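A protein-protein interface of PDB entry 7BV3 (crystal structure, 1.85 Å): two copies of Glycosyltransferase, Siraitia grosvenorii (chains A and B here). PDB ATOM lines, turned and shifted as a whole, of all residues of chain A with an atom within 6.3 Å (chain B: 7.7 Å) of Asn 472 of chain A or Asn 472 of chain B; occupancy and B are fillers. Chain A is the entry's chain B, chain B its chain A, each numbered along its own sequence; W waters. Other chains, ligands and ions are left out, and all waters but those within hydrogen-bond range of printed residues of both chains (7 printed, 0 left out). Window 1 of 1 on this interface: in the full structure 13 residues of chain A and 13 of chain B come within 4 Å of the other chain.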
ATOM      1  N   ARG A  28     -24.656  17.128 -13.312  1.00  0.00           N
ATOM      2  CA  ARG A  28     -25.003  17.826 -14.540  1.00  0.00           C
ATOM      3  C   ARG A  28     -26.478  18.180 -14.614  1.00  0.00           C
ATOM      4  O   ARG A  28     -26.846  19.063 -15.405  1.00  0.00           O
ATOM      5  CB  ARG A  28     -24.573  16.992 -15.748  1.00  0.00           C
ATOM      6  CG  ARG A  28     -23.058  17.094 -15.984  1.00  0.00           C
ATOM      7  CD  ARG A  28     -22.721  18.354 -16.788  1.00  0.00           C
ATOM      8  NE  ARG A  28     -23.251  18.193 -18.124  1.00  0.00           N
ATOM      9  CZ  ARG A  28     -22.587  17.594 -19.104  1.00  0.00           C
ATOM     10  NH1 ARG A  28     -21.343  17.145 -18.889  1.00  0.00           N
ATOM     11  NH2 ARG A  28     -23.158  17.446 -20.288  1.00  0.00           N
ATOM     12  N   SER A 467     -18.781  14.870 -26.215  1.00  0.00           N
ATOM     13  CA  SER A 467     -19.367  14.031 -25.169  1.00  0.00           C
ATOM     14  C   SER A 467     -20.222  14.841 -24.200  1.00  0.00           C
ATOM     15  O   SER A 467     -21.186  14.317 -23.636  1.00  0.00           O
ATOM     16  CB  SER A 467     -18.259  13.290 -24.408  1.00  0.00           C
ATOM     17  OG  SER A 467     -17.584  12.420 -25.299  1.00  0.00           O
ATOM     18  N   PHE A 468     -19.858  16.101 -23.963  1.00  0.00           N
ATOM     19  CA  PHE A 468     -20.702  16.993 -23.156  1.00  0.00           C
ATOM     20  C   PHE A 468     -22.105  17.108 -23.740  1.00  0.00           C
ATOM     21  O   PHE A 468     -23.104  16.937 -23.024  1.00  0.00           O
ATOM     22  CB  PHE A 468     -20.031  18.367 -23.058  1.00  0.00           C
ATOM     23  CG  PHE A 468     -20.818  19.408 -22.296  1.00  0.00           C
ATOM     24  CD1 PHE A 468     -20.629  19.583 -20.938  1.00  0.00           C
ATOM     25  CD2 PHE A 468     -21.676  20.264 -22.971  1.00  0.00           C
ATOM     26  CE1 PHE A 468     -21.331  20.565 -20.237  1.00  0.00           C
ATOM     27  CE2 PHE A 468     -22.395  21.257 -22.276  1.00  0.00           C
ATOM     28  CZ  PHE A 468     -22.215  21.399 -20.910  1.00  0.00           C
ATOM     29  N   THR A 469     -22.206  17.407 -25.038  1.00  0.00           N
ATOM     30  CA  THR A 469     -23.527  17.595 -25.622  1.00  0.00           C
ATOM     31  C   THR A 469     -24.229  16.263 -25.830  1.00  0.00           C
ATOM     32  O   THR A 469     -25.448  16.187 -25.692  1.00  0.00           O
ATOM     33  CB  THR A 469     -23.418  18.401 -26.925  1.00  0.00           C
ATOM     34  OG1 THR A 469     -22.807  17.614 -27.951  1.00  0.00           O
ATOM     35  CG2 THR A 469     -22.553  19.612 -26.682  1.00  0.00           C
ATOM     36  N   SER A 470     -23.482  15.184 -26.049  1.00  0.00           N
ATOM     37  CA  SER A 470     -24.122  13.874 -26.145  1.00  0.00           C
ATOM     38  C   SER A 470     -24.774  13.488 -24.820  1.00  0.00           C
ATOM     39  O   SER A 470     -25.884  12.934 -24.801  1.00  0.00           O
ATOM     40  CB  SER A 470     -23.071  12.831 -26.586  1.00  0.00           C
ATOM     41  OG  SER A 470     -23.661  11.562 -26.803  1.00  0.00           O
ATOM     42  N   LEU A 471     -24.114  13.784 -23.694  1.00  0.00           N
ATOM     43  CA  LEU A 471     -24.739  13.491 -22.405  1.00  0.00           C
ATOM     44  C   LEU A 471     -25.983  14.362 -22.188  1.00  0.00           C
ATOM     45  O   LEU A 471     -26.961  13.926 -21.576  1.00  0.00           O
ATOM     46  CB  LEU A 471     -23.728  13.701 -21.275  1.00  0.00           C
ATOM     47  CG  LEU A 471     -24.174  13.207 -19.897  1.00  0.00           C
ATOM     48  CD1 LEU A 471     -24.009  11.683 -19.787  1.00  0.00           C
ATOM     49  CD2 LEU A 471     -23.395  13.909 -18.807  1.00  0.00           C
ATOM     50  N   ASN A 472     -25.954  15.598 -22.675  1.00  0.00           N
ATOM     51  CA  ASN A 472     -27.135  16.451 -22.555  1.00  0.00           C
ATOM     52  C   ASN A 472     -28.313  15.868 -23.329  1.00  0.00           C
ATOM     53  O   ASN A 472     -29.471  15.955 -22.887  1.00  0.00           O
ATOM     54  CB  ASN A 472     -26.802  17.863 -23.042  1.00  0.00           C
ATOM     55  CG  ASN A 472     -25.901  18.596 -22.079  1.00  0.00           C
ATOM     56  OD1 ASN A 472     -25.833  18.246 -20.900  1.00  0.00           O
ATOM     57  ND2 ASN A 472     -25.244  19.649 -22.554  1.00  0.00           N
ATOM     58  N   ARG A 473     -28.048  15.320 -24.509  1.00  0.00           N
ATOM     59  CA  ARG A 473     -29.120  14.709 -25.280  1.00  0.00           C
ATOM     60  C   ARG A 473     -29.716  13.524 -24.546  1.00  0.00           C
ATOM     61  O   ARG A 473     -30.933  13.331 -24.563  1.00  0.00           O
ATOM     62  CB  ARG A 473     -28.617  14.298 -26.658  1.00  0.00           C
ATOM     63  CG  ARG A 473     -28.419  15.465 -27.600  1.00  0.00           C
ATOM     64  CD  ARG A 473     -28.205  14.993 -29.038  1.00  0.00           C
ATOM     65  NE  ARG A 473     -27.021  14.125 -29.187  1.00  0.00           N
ATOM     66  CZ  ARG A 473     -25.778  14.573 -29.331  1.00  0.00           C
ATOM     67  NH1 ARG A 473     -25.527  15.871 -29.335  1.00  0.00           N
ATOM     68  NH2 ARG A 473     -24.766  13.706 -29.462  1.00  0.00           N
ATOM     69  N   PHE A 474     -28.872  12.700 -23.913  1.00  0.00           N
ATOM     70  CA  PHE A 474     -29.387  11.628 -23.070  1.00  0.00           C
ATOM     71  C   PHE A 474     -30.205  12.182 -21.909  1.00  0.00           C
ATOM     72  O   PHE A 474     -31.312  11.699 -21.627  1.00  0.00           O
ATOM     73  CB  PHE A 474     -28.214  10.781 -22.551  1.00  0.00           C
ATOM     74  CG  PHE A 474     -28.604   9.817 -21.465  1.00  0.00           C
ATOM     75  CD1 PHE A 474     -29.349   8.695 -21.762  1.00  0.00           C
ATOM     76  CD2 PHE A 474     -28.240  10.057 -20.149  1.00  0.00           C
ATOM     77  CE1 PHE A 474     -29.709   7.808 -20.772  1.00  0.00           C
ATOM     78  CE2 PHE A 474     -28.600   9.171 -19.150  1.00  0.00           C
ATOM     79  CZ  PHE A 474     -29.353   8.051 -19.467  1.00  0.00           C
ATOM     80  N   ILE A 475     -29.687  13.201 -21.224  1.00  0.00           N
ATOM     81  CA  ILE A 475     -30.423  13.760 -20.091  1.00  0.00           C
ATOM     82  C   ILE A 475     -31.766  14.300 -20.547  1.00  0.00           C
ATOM     83  O   ILE A 475     -32.782  14.098 -19.883  1.00  0.00           O
ATOM     84  CB  ILE A 475     -29.603  14.847 -19.379  1.00  0.00           C
ATOM     85  CG1 ILE A 475     -28.425  14.230 -18.634  1.00  0.00           C
ATOM     86  CG2 ILE A 475     -30.476  15.612 -18.388  1.00  0.00           C
ATOM     87  CD1 ILE A 475     -27.365  15.242 -18.256  1.00  0.00           C
ATOM     88  N   ASP A 476     -31.798  14.943 -21.714  1.00  0.00           N
ATOM     89  CA  ASP A 476     -33.065  15.448 -22.236  1.00  0.00           C
ATOM     90  C   ASP A 476     -34.064  14.316 -22.442  1.00  0.00           C
ATOM     91  O   ASP A 476     -35.212  14.408 -21.997  1.00  0.00           O
ATOM     92  CB  ASP A 476     -32.834  16.188 -23.547  1.00  0.00           C
ATOM     93  CG  ASP A 476     -32.165  17.531 -23.348  1.00  0.00           C
ATOM     94  OD1 ASP A 476     -32.085  18.022 -22.202  1.00  0.00           O
ATOM     95  OD2 ASP A 476     -31.736  18.109 -24.361  1.00  0.00           O
ATOM     96  N   GLU A 477     -33.640  13.233 -23.106  1.00  0.00           N
ATOM     97  CA  GLU A 477     -34.518  12.083 -23.324  1.00  0.00           C
ATOM     98  C   GLU A 477     -35.046  11.543 -22.001  1.00  0.00           C
ATOM     99  O   GLU A 477     -36.242  11.267 -21.855  1.00  0.00           O
ATOM    100  CB  GLU A 477     -33.756  10.991 -24.091  1.00  0.00           C
ATOM    101  CG  GLU A 477     -34.534   9.694 -24.312  1.00  0.00           C
ATOM    102  CD  GLU A 477     -35.701   9.844 -25.277  1.00  0.00           C
ATOM    103  OE1 GLU A 477     -35.703  10.803 -26.083  1.00  0.00           O
ATOM    104  OE2 GLU A 477     -36.602   8.979 -25.246  1.00  0.00           O
ATOM    105  N   LEU B  24     -22.937  32.524 -24.542  1.00  0.00           N
ATOM    106  CA  LEU B  24     -23.283  31.332 -23.771  1.00  0.00           C
ATOM    107  C   LEU B  24     -23.573  30.150 -24.679  1.00  0.00           C
ATOM    108  O   LEU B  24     -23.087  29.037 -24.442  1.00  0.00           O
ATOM    109  CB  LEU B  24     -24.499  31.605 -22.894  1.00  0.00           C
ATOM    110  CG  LEU B  24     -24.362  31.983 -21.434  1.00  0.00           C
ATOM    111  CD1 LEU B  24     -25.725  32.411 -20.960  1.00  0.00           C
ATOM    112  CD2 LEU B  24     -23.841  30.789 -20.628  1.00  0.00           C
ATOM    113  N   LEU B  25     -24.408  30.365 -25.697  1.00  0.00           N
ATOM    114  CA  LEU B  25     -24.751  29.291 -26.621  1.00  0.00           C
ATOM    115  C   LEU B  25     -23.513  28.753 -27.313  1.00  0.00           C
ATOM    116  O   LEU B  25     -23.354  27.534 -27.463  1.00  0.00           O
ATOM    117  CB  LEU B  25     -25.756  29.794 -27.660  1.00  0.00           C
ATOM    118  CG  LEU B  25     -27.164  30.146 -27.166  1.00  0.00           C
ATOM    119  CD1 LEU B  25     -27.941  30.827 -28.275  1.00  0.00           C
ATOM    120  CD2 LEU B  25     -27.904  28.894 -26.697  1.00  0.00           C
ATOM    121  N   ARG B  28     -21.467  26.572 -25.085  1.00  0.00           N
ATOM    122  CA  ARG B  28     -22.129  25.331 -24.698  1.00  0.00           C
ATOM    123  C   ARG B  28     -22.235  24.313 -25.812  1.00  0.00           C
ATOM    124  O   ARG B  28     -22.567  23.157 -25.532  1.00  0.00           O
ATOM    125  CB  ARG B  28     -23.545  25.594 -24.216  1.00  0.00           C
ATOM    126  CG  ARG B  28     -23.606  26.256 -22.933  1.00  0.00           C
ATOM    127  CD  ARG B  28     -23.261  25.319 -21.785  1.00  0.00           C
ATOM    128  NE  ARG B  28     -23.378  26.179 -20.645  1.00  0.00           N
ATOM    129  CZ  ARG B  28     -24.545  26.443 -20.078  1.00  0.00           C
ATOM    130  NH1 ARG B  28     -25.659  25.824 -20.508  1.00  0.00           N
ATOM    131  NH2 ARG B  28     -24.576  27.295 -19.077  1.00  0.00           N
ATOM    132  N   ASP B  29     -22.034  24.709 -27.061  1.00  0.00           N
ATOM    133  CA  ASP B  29     -22.038  23.725 -28.135  1.00  0.00           C
ATOM    134  C   ASP B  29     -21.074  24.203 -29.208  1.00  0.00           C
ATOM    135  O   ASP B  29     -21.361  25.163 -29.928  1.00  0.00           O
ATOM    136  CB  ASP B  29     -23.447  23.513 -28.681  1.00  0.00           C
ATOM    137  CG  ASP B  29     -23.533  22.320 -29.619  1.00  0.00           C
ATOM    138  OD1 ASP B  29     -22.482  21.858 -30.111  1.00  0.00           O
ATOM    139  OD2 ASP B  29     -24.655  21.816 -29.837  1.00  0.00           O
ATOM    140  N   TYR B 240     -38.224  28.493 -22.207  1.00  0.00           N
ATOM    141  CA  TYR B 240     -36.959  28.129 -21.563  1.00  0.00           C
ATOM    142  C   TYR B 240     -36.527  29.280 -20.669  1.00  0.00           C
ATOM    143  O   TYR B 240     -36.163  30.351 -21.168  1.00  0.00           O
ATOM    144  CB  TYR B 240     -35.865  27.854 -22.594  1.00  0.00           C
ATOM    145  CG  TYR B 240     -36.206  26.817 -23.616  1.00  0.00           C
ATOM    146  CD1 TYR B 240     -35.863  25.478 -23.420  1.00  0.00           C
ATOM    147  CD2 TYR B 240     -36.855  27.171 -24.792  1.00  0.00           C
ATOM    148  CE1 TYR B 240     -36.167  24.513 -24.381  1.00  0.00           C
ATOM    149  CE2 TYR B 240     -37.180  26.215 -25.745  1.00  0.00           C
ATOM    150  CZ  TYR B 240     -36.817  24.897 -25.541  1.00  0.00           C
ATOM    151  OH  TYR B 240     -37.150  23.973 -26.495  1.00  0.00           O
ATOM    152  N   VAL B 242     -33.729  30.800 -18.888  1.00  0.00           N
ATOM    153  CA  VAL B 242     -32.298  30.599 -19.068  1.00  0.00           C
ATOM    154  C   VAL B 242     -31.472  31.683 -18.388  1.00  0.00           C
ATOM    155  O   VAL B 242     -30.256  31.726 -18.564  1.00  0.00           O
ATOM    156  CB  VAL B 242     -31.929  30.493 -20.564  1.00  0.00           C
ATOM    157  CG1 VAL B 242     -32.621  29.288 -21.183  1.00  0.00           C
ATOM    158  CG2 VAL B 242     -32.308  31.765 -21.308  1.00  0.00           C
ATOM    159  N   GLU B 463     -23.446  24.784 -13.274  1.00  0.00           N
ATOM    160  CA  GLU B 463     -23.629  23.408 -13.721  1.00  0.00           C
ATOM    161  C   GLU B 463     -24.706  22.705 -12.909  1.00  0.00           C
ATOM    162  O   GLU B 463     -24.733  22.796 -11.678  1.00  0.00           O
ATOM    163  CB  GLU B 463     -22.296  22.629 -13.610  1.00  0.00           C
ATOM    164  CG  GLU B 463     -22.385  21.237 -14.247  1.00  0.00           C
ATOM    165  CD  GLU B 463     -21.200  20.320 -13.866  1.00  0.00           C
ATOM    166  OE1 GLU B 463     -20.496  20.587 -12.875  1.00  0.00           O
ATOM    167  OE2 GLU B 463     -20.978  19.325 -14.566  1.00  0.00           O
ATOM    168  N   GLY B 464     -25.624  22.035 -13.606  1.00  0.00           N
ATOM    169  CA  GLY B 464     -26.717  21.329 -12.971  1.00  0.00           C
ATOM    170  C   GLY B 464     -27.949  22.167 -12.653  1.00  0.00           C
ATOM    171  O   GLY B 464     -29.026  21.598 -12.439  1.00  0.00           O
ATOM    172  N   GLY B 465     -27.818  23.491 -12.616  1.00  0.00           N
ATOM    173  CA  GLY B 465     -28.938  24.357 -12.241  1.00  0.00           C
ATOM    174  C   GLY B 465     -30.027  24.440 -13.301  1.00  0.00           C
ATOM    175  O   GLY B 465     -29.861  24.049 -14.453  1.00  0.00           O
ATOM    176  N   SER B 466     -31.175  25.003 -12.898  1.00  0.00           N
ATOM    177  CA  SER B 466     -32.348  25.007 -13.768  1.00  0.00           C
ATOM    178  C   SER B 466     -32.091  25.747 -15.080  1.00  0.00           C
ATOM    179  O   SER B 466     -32.486  25.268 -16.147  1.00  0.00           O
ATOM    180  CB  SER B 466     -33.548  25.626 -13.026  1.00  0.00           C
ATOM    181  OG  SER B 466     -33.239  26.956 -12.618  1.00  0.00           O
ATOM    182  N   SER B 467     -31.437  26.910 -15.034  1.00  0.00           N
ATOM    183  CA  SER B 467     -31.224  27.650 -16.275  1.00  0.00           C
ATOM    184  C   SER B 467     -30.098  27.063 -17.101  1.00  0.00           C
ATOM    185  O   SER B 467     -30.146  27.121 -18.332  1.00  0.00           O
ATOM    186  CB  SER B 467     -30.938  29.137 -15.986  1.00  0.00           C
ATOM    187  OG  SER B 467     -32.037  29.709 -15.285  1.00  0.00           O
ATOM    188  N   PHE B 468     -29.102  26.483 -16.437  1.00  0.00           N
ATOM    189  CA  PHE B 468     -28.047  25.747 -17.136  1.00  0.00           C
ATOM    190  C   PHE B 468     -28.635  24.599 -17.957  1.00  0.00           C
ATOM    191  O   PHE B 468     -28.369  24.468 -19.158  1.00  0.00           O
ATOM    192  CB  PHE B 468     -27.052  25.236 -16.092  1.00  0.00           C
ATOM    193  CG  PHE B 468     -25.848  24.520 -16.661  1.00  0.00           C
ATOM    194  CD1 PHE B 468     -24.690  25.206 -16.933  1.00  0.00           C
ATOM    195  CD2 PHE B 468     -25.886  23.153 -16.859  1.00  0.00           C
ATOM    196  CE1 PHE B 468     -23.555  24.536 -17.432  1.00  0.00           C
ATOM    197  CE2 PHE B 468     -24.752  22.476 -17.366  1.00  0.00           C
ATOM    198  CZ  PHE B 468     -23.608  23.180 -17.647  1.00  0.00           C
ATOM    199  N   THR B 469     -29.458  23.763 -17.331  1.00  0.00           N
ATOM    200  CA  THR B 469     -30.027  22.640 -18.070  1.00  0.00           C
ATOM    201  C   THR B 469     -31.094  23.089 -19.062  1.00  0.00           C
ATOM    202  O   THR B 469     -31.240  22.476 -20.127  1.00  0.00           O
ATOM    203  CB  THR B 469     -30.594  21.593 -17.110  1.00  0.00           C
ATOM    204  OG1 THR B 469     -31.643  22.170 -16.321  1.00  0.00           O
ATOM    205  CG2 THR B 469     -29.483  21.044 -16.205  1.00  0.00           C
ATOM    206  N   SER B 470     -31.850  24.148 -18.754  1.00  0.00           N
ATOM    207  CA  SER B 470     -32.831  24.602 -19.737  1.00  0.00           C
ATOM    208  C   SER B 470     -32.154  25.128 -20.993  1.00  0.00           C
ATOM    209  O   SER B 470     -32.630  24.901 -22.107  1.00  0.00           O
ATOM    210  CB  SER B 470     -33.716  25.702 -19.115  1.00  0.00           C
ATOM    211  OG  SER B 470     -34.655  25.128 -18.218  1.00  0.00           O
ATOM    212  N   LEU B 471     -31.034  25.827 -20.837  1.00  0.00           N
ATOM    213  CA  LEU B 471     -30.288  26.262 -22.010  1.00  0.00           C
ATOM    214  C   LEU B 471     -29.771  25.068 -22.817  1.00  0.00           C
ATOM    215  O   LEU B 471     -29.807  25.074 -24.060  1.00  0.00           O
ATOM    216  CB  LEU B 471     -29.144  27.183 -21.585  1.00  0.00           C
ATOM    217  CG  LEU B 471     -28.467  27.938 -22.736  1.00  0.00           C
ATOM    218  CD1 LEU B 471     -29.431  28.964 -23.282  1.00  0.00           C
ATOM    219  CD2 LEU B 471     -27.176  28.610 -22.310  1.00  0.00           C
ATOM    220  N   ASN B 472     -29.266  24.034 -22.135  1.00  0.00           N
ATOM    221  CA  ASN B 472     -28.854  22.826 -22.851  1.00  0.00           C
ATOM    222  C   ASN B 472     -30.010  22.197 -23.616  1.00  0.00           C
ATOM    223  O   ASN B 472     -29.821  21.688 -24.729  1.00  0.00           O
ATOM    224  CB  ASN B 472     -28.267  21.796 -21.873  1.00  0.00           C
ATOM    225  CG  ASN B 472     -26.963  22.249 -21.270  1.00  0.00           C
ATOM    226  OD1 ASN B 472     -26.240  23.063 -21.853  1.00  0.00           O
ATOM    227  ND2 ASN B 472     -26.620  21.687 -20.104  1.00  0.00           N
ATOM    228  N   ARG B 473     -31.206  22.173 -23.016  1.00  0.00           N
ATOM    229  CA  ARG B 473     -32.354  21.594 -23.702  1.00  0.00           C
ATOM    230  C   ARG B 473     -32.718  22.399 -24.943  1.00  0.00           C
ATOM    231  O   ARG B 473     -33.050  21.825 -25.991  1.00  0.00           O
ATOM    232  CB  ARG B 473     -33.548  21.506 -22.739  1.00  0.00           C
ATOM    233  CG  ARG B 473     -34.801  20.895 -23.337  1.00  0.00           C
ATOM    234  CD  ARG B 473     -35.853  20.600 -22.243  1.00  0.00           C
ATOM    235  NE  ARG B 473     -36.304  21.817 -21.556  1.00  0.00           N
ATOM    236  CZ  ARG B 473     -35.897  22.193 -20.342  1.00  0.00           C
ATOM    237  NH1 ARG B 473     -35.012  21.465 -19.666  1.00  0.00           N
ATOM    238  NH2 ARG B 473     -36.362  23.320 -19.802  1.00  0.00           N
ATOM    239  N   PHE B 474     -32.676  23.735 -24.845  1.00  0.00           N
ATOM    240  CA  PHE B 474     -32.891  24.568 -26.029  1.00  0.00           C
ATOM    241  C   PHE B 474     -31.870  24.254 -27.132  1.00  0.00           C
ATOM    242  O   PHE B 474     -32.232  24.066 -28.302  1.00  0.00           O
ATOM    243  CB  PHE B 474     -32.811  26.048 -25.636  1.00  0.00           C
ATOM    244  CG  PHE B 474     -32.744  26.991 -26.816  1.00  0.00           C
ATOM    245  CD1 PHE B 474     -33.881  27.274 -27.563  1.00  0.00           C
ATOM    246  CD2 PHE B 474     -31.553  27.610 -27.157  1.00  0.00           C
ATOM    247  CE1 PHE B 474     -33.808  28.145 -28.648  1.00  0.00           C
ATOM    248  CE2 PHE B 474     -31.474  28.469 -28.238  1.00  0.00           C
ATOM    249  CZ  PHE B 474     -32.607  28.741 -28.979  1.00  0.00           C
ATOM    250  N   ILE B 475     -30.583  24.226 -26.781  1.00  0.00           N
ATOM    251  CA  ILE B 475     -29.532  23.921 -27.763  1.00  0.00           C
ATOM    252  C   ILE B 475     -29.795  22.584 -28.438  1.00  0.00           C
ATOM    253  O   ILE B 475     -29.663  22.446 -29.665  1.00  0.00           O
ATOM    254  CB  ILE B 475     -28.147  23.914 -27.091  1.00  0.00           C
ATOM    255  CG1 ILE B 475     -27.712  25.320 -26.738  1.00  0.00           C
ATOM    256  CG2 ILE B 475     -27.097  23.210 -27.987  1.00  0.00           C
ATOM    257  CD1 ILE B 475     -26.521  25.329 -25.788  1.00  0.00           C
ATOM    258  N   ASP B 476     -30.165  21.576 -27.649  1.00  0.00           N
ATOM    259  CA  ASP B 476     -30.419  20.258 -28.218  1.00  0.00           C
ATOM    260  C   ASP B 476     -31.602  20.287 -29.183  1.00  0.00           C
ATOM    261  O   ASP B 476     -31.547  19.675 -30.255  1.00  0.00           O
ATOM    262  CB  ASP B 476     -30.630  19.242 -27.093  1.00  0.00           C
ATOM    263  CG  ASP B 476     -29.353  19.030 -26.259  1.00  0.00           C
ATOM    264  OD1 ASP B 476     -28.259  19.388 -26.740  1.00  0.00           O
ATOM    265  OD2 ASP B 476     -29.417  18.514 -25.127  1.00  0.00           O
ATOM    266  N   GLU B 477     -32.671  21.013 -28.837  1.00  0.00           N
ATOM    267  CA  GLU B 477     -33.779  21.192 -29.780  1.00  0.00           C
ATOM    268  C   GLU B 477     -33.314  21.871 -31.062  1.00  0.00           C
ATOM    269  O   GLU B 477     -33.626  21.416 -32.169  1.00  0.00           O
ATOM    270  CB  GLU B 477     -34.904  22.009 -29.136  1.00  0.00           C
ATOM    271  CG  GLU B 477     -35.736  21.208 -28.172  1.00  0.00           C
ATOM    272  CD  GLU B 477     -36.484  20.087 -28.875  1.00  0.00           C
ATOM    273  OE1 GLU B 477     -36.904  20.297 -30.034  1.00  0.00           O
ATOM    274  OE2 GLU B 477     -36.632  19.000 -28.280  1.00  0.00           O
ATOM    275  N   VAL B 478     -32.572  22.969 -30.925  1.00  0.00           N
ATOM    276  CA  VAL B 478     -32.070  23.713 -32.079  1.00  0.00           C
ATOM    277  C   VAL B 478     -31.243  22.817 -32.988  1.00  0.00           C
ATOM    278  O   VAL B 478     -31.332  22.905 -34.221  1.00  0.00           O
ATOM    279  CB  VAL B 478     -31.251  24.928 -31.601  1.00  0.00           C
ATOM    280  CG1 VAL B 478     -30.389  25.481 -32.709  1.00  0.00           C
ATOM    281  CG2 VAL B 478     -32.177  26.012 -31.047  1.00  0.00           C
ATOM    282  N   MET B 479     -30.416  21.952 -32.400  1.00  0.00           N
ATOM    283  CA  MET B 479     -29.477  21.156 -33.173  1.00  0.00           C
ATOM    284  C   MET B 479     -30.096  19.888 -33.739  1.00  0.00           C
ATOM    285  O   MET B 479     -29.411  19.159 -34.460  1.00  0.00           O
ATOM    286  CB  MET B 479     -28.260  20.811 -32.319  1.00  0.00           C
ATOM    287  CG  MET B 479     -27.439  22.034 -31.935  1.00  0.00           C
ATOM    288  SD  MET B 479     -26.868  22.993 -33.372  1.00  0.00           S
ATOM    289  CE  MET B 479     -25.611  21.892 -33.984  1.00  0.00           C
HETATM  290  O   HOH W   1     -19.347  18.075 -16.855  1.00  0.00           O
HETATM  291  O   HOH W   2     -27.308  18.244 -29.332  1.00  0.00           O
HETATM  292  O   HOH W   3     -34.042  18.571 -20.170  1.00  0.00           O
HETATM  293  O   HOH W   4     -30.794  19.528 -20.425  1.00  0.00           O
HETATM  294  O   HOH W   5     -20.824  19.613 -29.335  1.00  0.00           O
HETATM  295  O   HOH W   6     -25.816  19.504 -18.015  1.00  0.00           O
HETATM  296  O   HOH W   7     -28.158  19.581 -19.380  1.00  0.00           O
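The side-chain amide nitrogen (ND2) of Asn 472 of chain B lies close to the side-chain amide nitrogen (ND2) of Asn 472 of chain A (3.5 Å).
OD2 of Asp 476 of chain B sits close to O of Asn 472 of chain A (3.4 Å).
OD2 of Asp 476 of chain B lies close to OD2 of Asp 476 of chain A.
O of Phe 468 of chain B lies close to ND2 of Asn 472 of chain B, at 3.4 Å.
NH1 of Arg 28 of chain B sits at hydrogen-bond distance from O of Phe 468 of chain B.
O of Gly 465 of chain B sits at hydrogen-bond distance from OG1 of Thr 469 of chain B (3.2 Å).
NH2 of Arg 28 of chain A lies within hydrogen-bond range of O of Phe 468 of chain A, at 2.8 Å.
The guanidinium group (NH1) of Arg 28 of chain B lies within hydrogen-bond range of the side-chain amide oxygen (OD1) of Asn 472 of chain B, 3.1 Å away.
The side-chain amide nitrogen (ND2) of Asn 472 of chain A sits close to the backbone carbonyl oxygen (O) of Phe 468 of chain A (3.5 Å).
Among the printed residues, merely in contact across the chains: Arg 28 of chain A with Glu 463 of chain B (3.0 Å), Arg 28 of chain A with Gly 464 of chain B (3.3 Å), Arg 28 of chain A with Thr 469 of chain B (3.4 Å), Arg 473 of chain A with Asp 476 of chain B (3.5 Å), Asp 476 of chain A with Arg 473 of chain B (3.6 Å), Thr 469 of chain A with Arg 28 of chain B (3.7 Å), Phe 468 of chain A with Arg 28 of chain B (3.8 Å) and Phe 468 of chain A with Phe 468 of chain B (3.97 Å).
Of the printed residues of chain B, Phe 468 of chain A touches Arg 28 (3.8 Å) and Phe 468 (3.97 Å).
Printed residues of chain B within 4 Å of Asn 472 of chain A: Asn 472 (3.4 Å) and Asp 476 (3.4 Å).
Of the printed residues of chain B, Asp 476 of chain A touches Arg 473 (3.6 Å) and Asp 476 (2.5 Å).
Printed residues of chain A within 4 Å of Arg 28 of chain B: Phe 468 (3.8 Å) and Thr 469 (3.7 Å).
Of the printed residues of chain A, Thr 469 of chain B touches Arg 28.
Of chain A, only Asn 472 comes within 4 Å of Asn 472 of chain B.
Of the printed residues of chain A, Arg 473 of chain B touches Asp 476 (3.6 Å).
The nearest printed residue of chain B that does not touch Thr 469 of chain A is Asp 29 of chain B (4.1 Å).
Hydrophobic or aromatic side chains of chain B that line the printed part of chain A: Phe 468.
Hydrophobic or aromatic side chains of chain A within 4 Å of the printed part of chain B: Phe 468.
Among the printed residues, 11 pairs touch across the chains.
Among the printed residues, no Asp or Glu carboxylate lies within 4 Å of a Lys or Arg side-chain nitrogen of the other chain.
Phe 468 of chain B touches its own counterpart, Phe 468 of chain A.
Asn 472 of chain B touches its own counterpart, Asn 472 of chain A.
Asn 472 of chain A touches Asp 476 of chain B, but with the chains exchanged Asp 476 of chain A does not touch Asn 472 of chain B (4.1 Å).
Asp 476 of chain B touches its own counterpart, Asp 476 of chain A.
12 positions are printed for both chains.
Water W4 bridges OD1 of Asp 476 of chain A and O of Thr 469 of chain B.
Water W7 bridges the side-chain amide nitrogen of Asn 472 of chain B (2.7 Å) and the side-chain amide oxygen of Asn 472 of chain A (3.1 Å).
Water W6 lies within hydrogen-bond range of O of Arg 28 of chain A (2.8 Å), ND2 of Asn 472 of chain B (3.1 Å) and OD1 of Asn 472 of chain A (3.1 Å).
Water W3 bridges the side-chain carboxylate of Asp 476 of chain A and the guanidinium group of Arg 473 of chain B.
Water W2 lies within hydrogen-bond range of the guanidinium group (NH1) of Arg 473 of chain A (3.0 Å) and the side-chain carboxylate (OD1) of Asp 476 of chain B (3.0 Å).
Water W1 lies within hydrogen-bond range of the guanidinium group (NH1) of Arg 28 of chain A (3.0 Å) and the side-chain carboxylate (OE2) of Glu 463 of chain B (3.1 Å).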
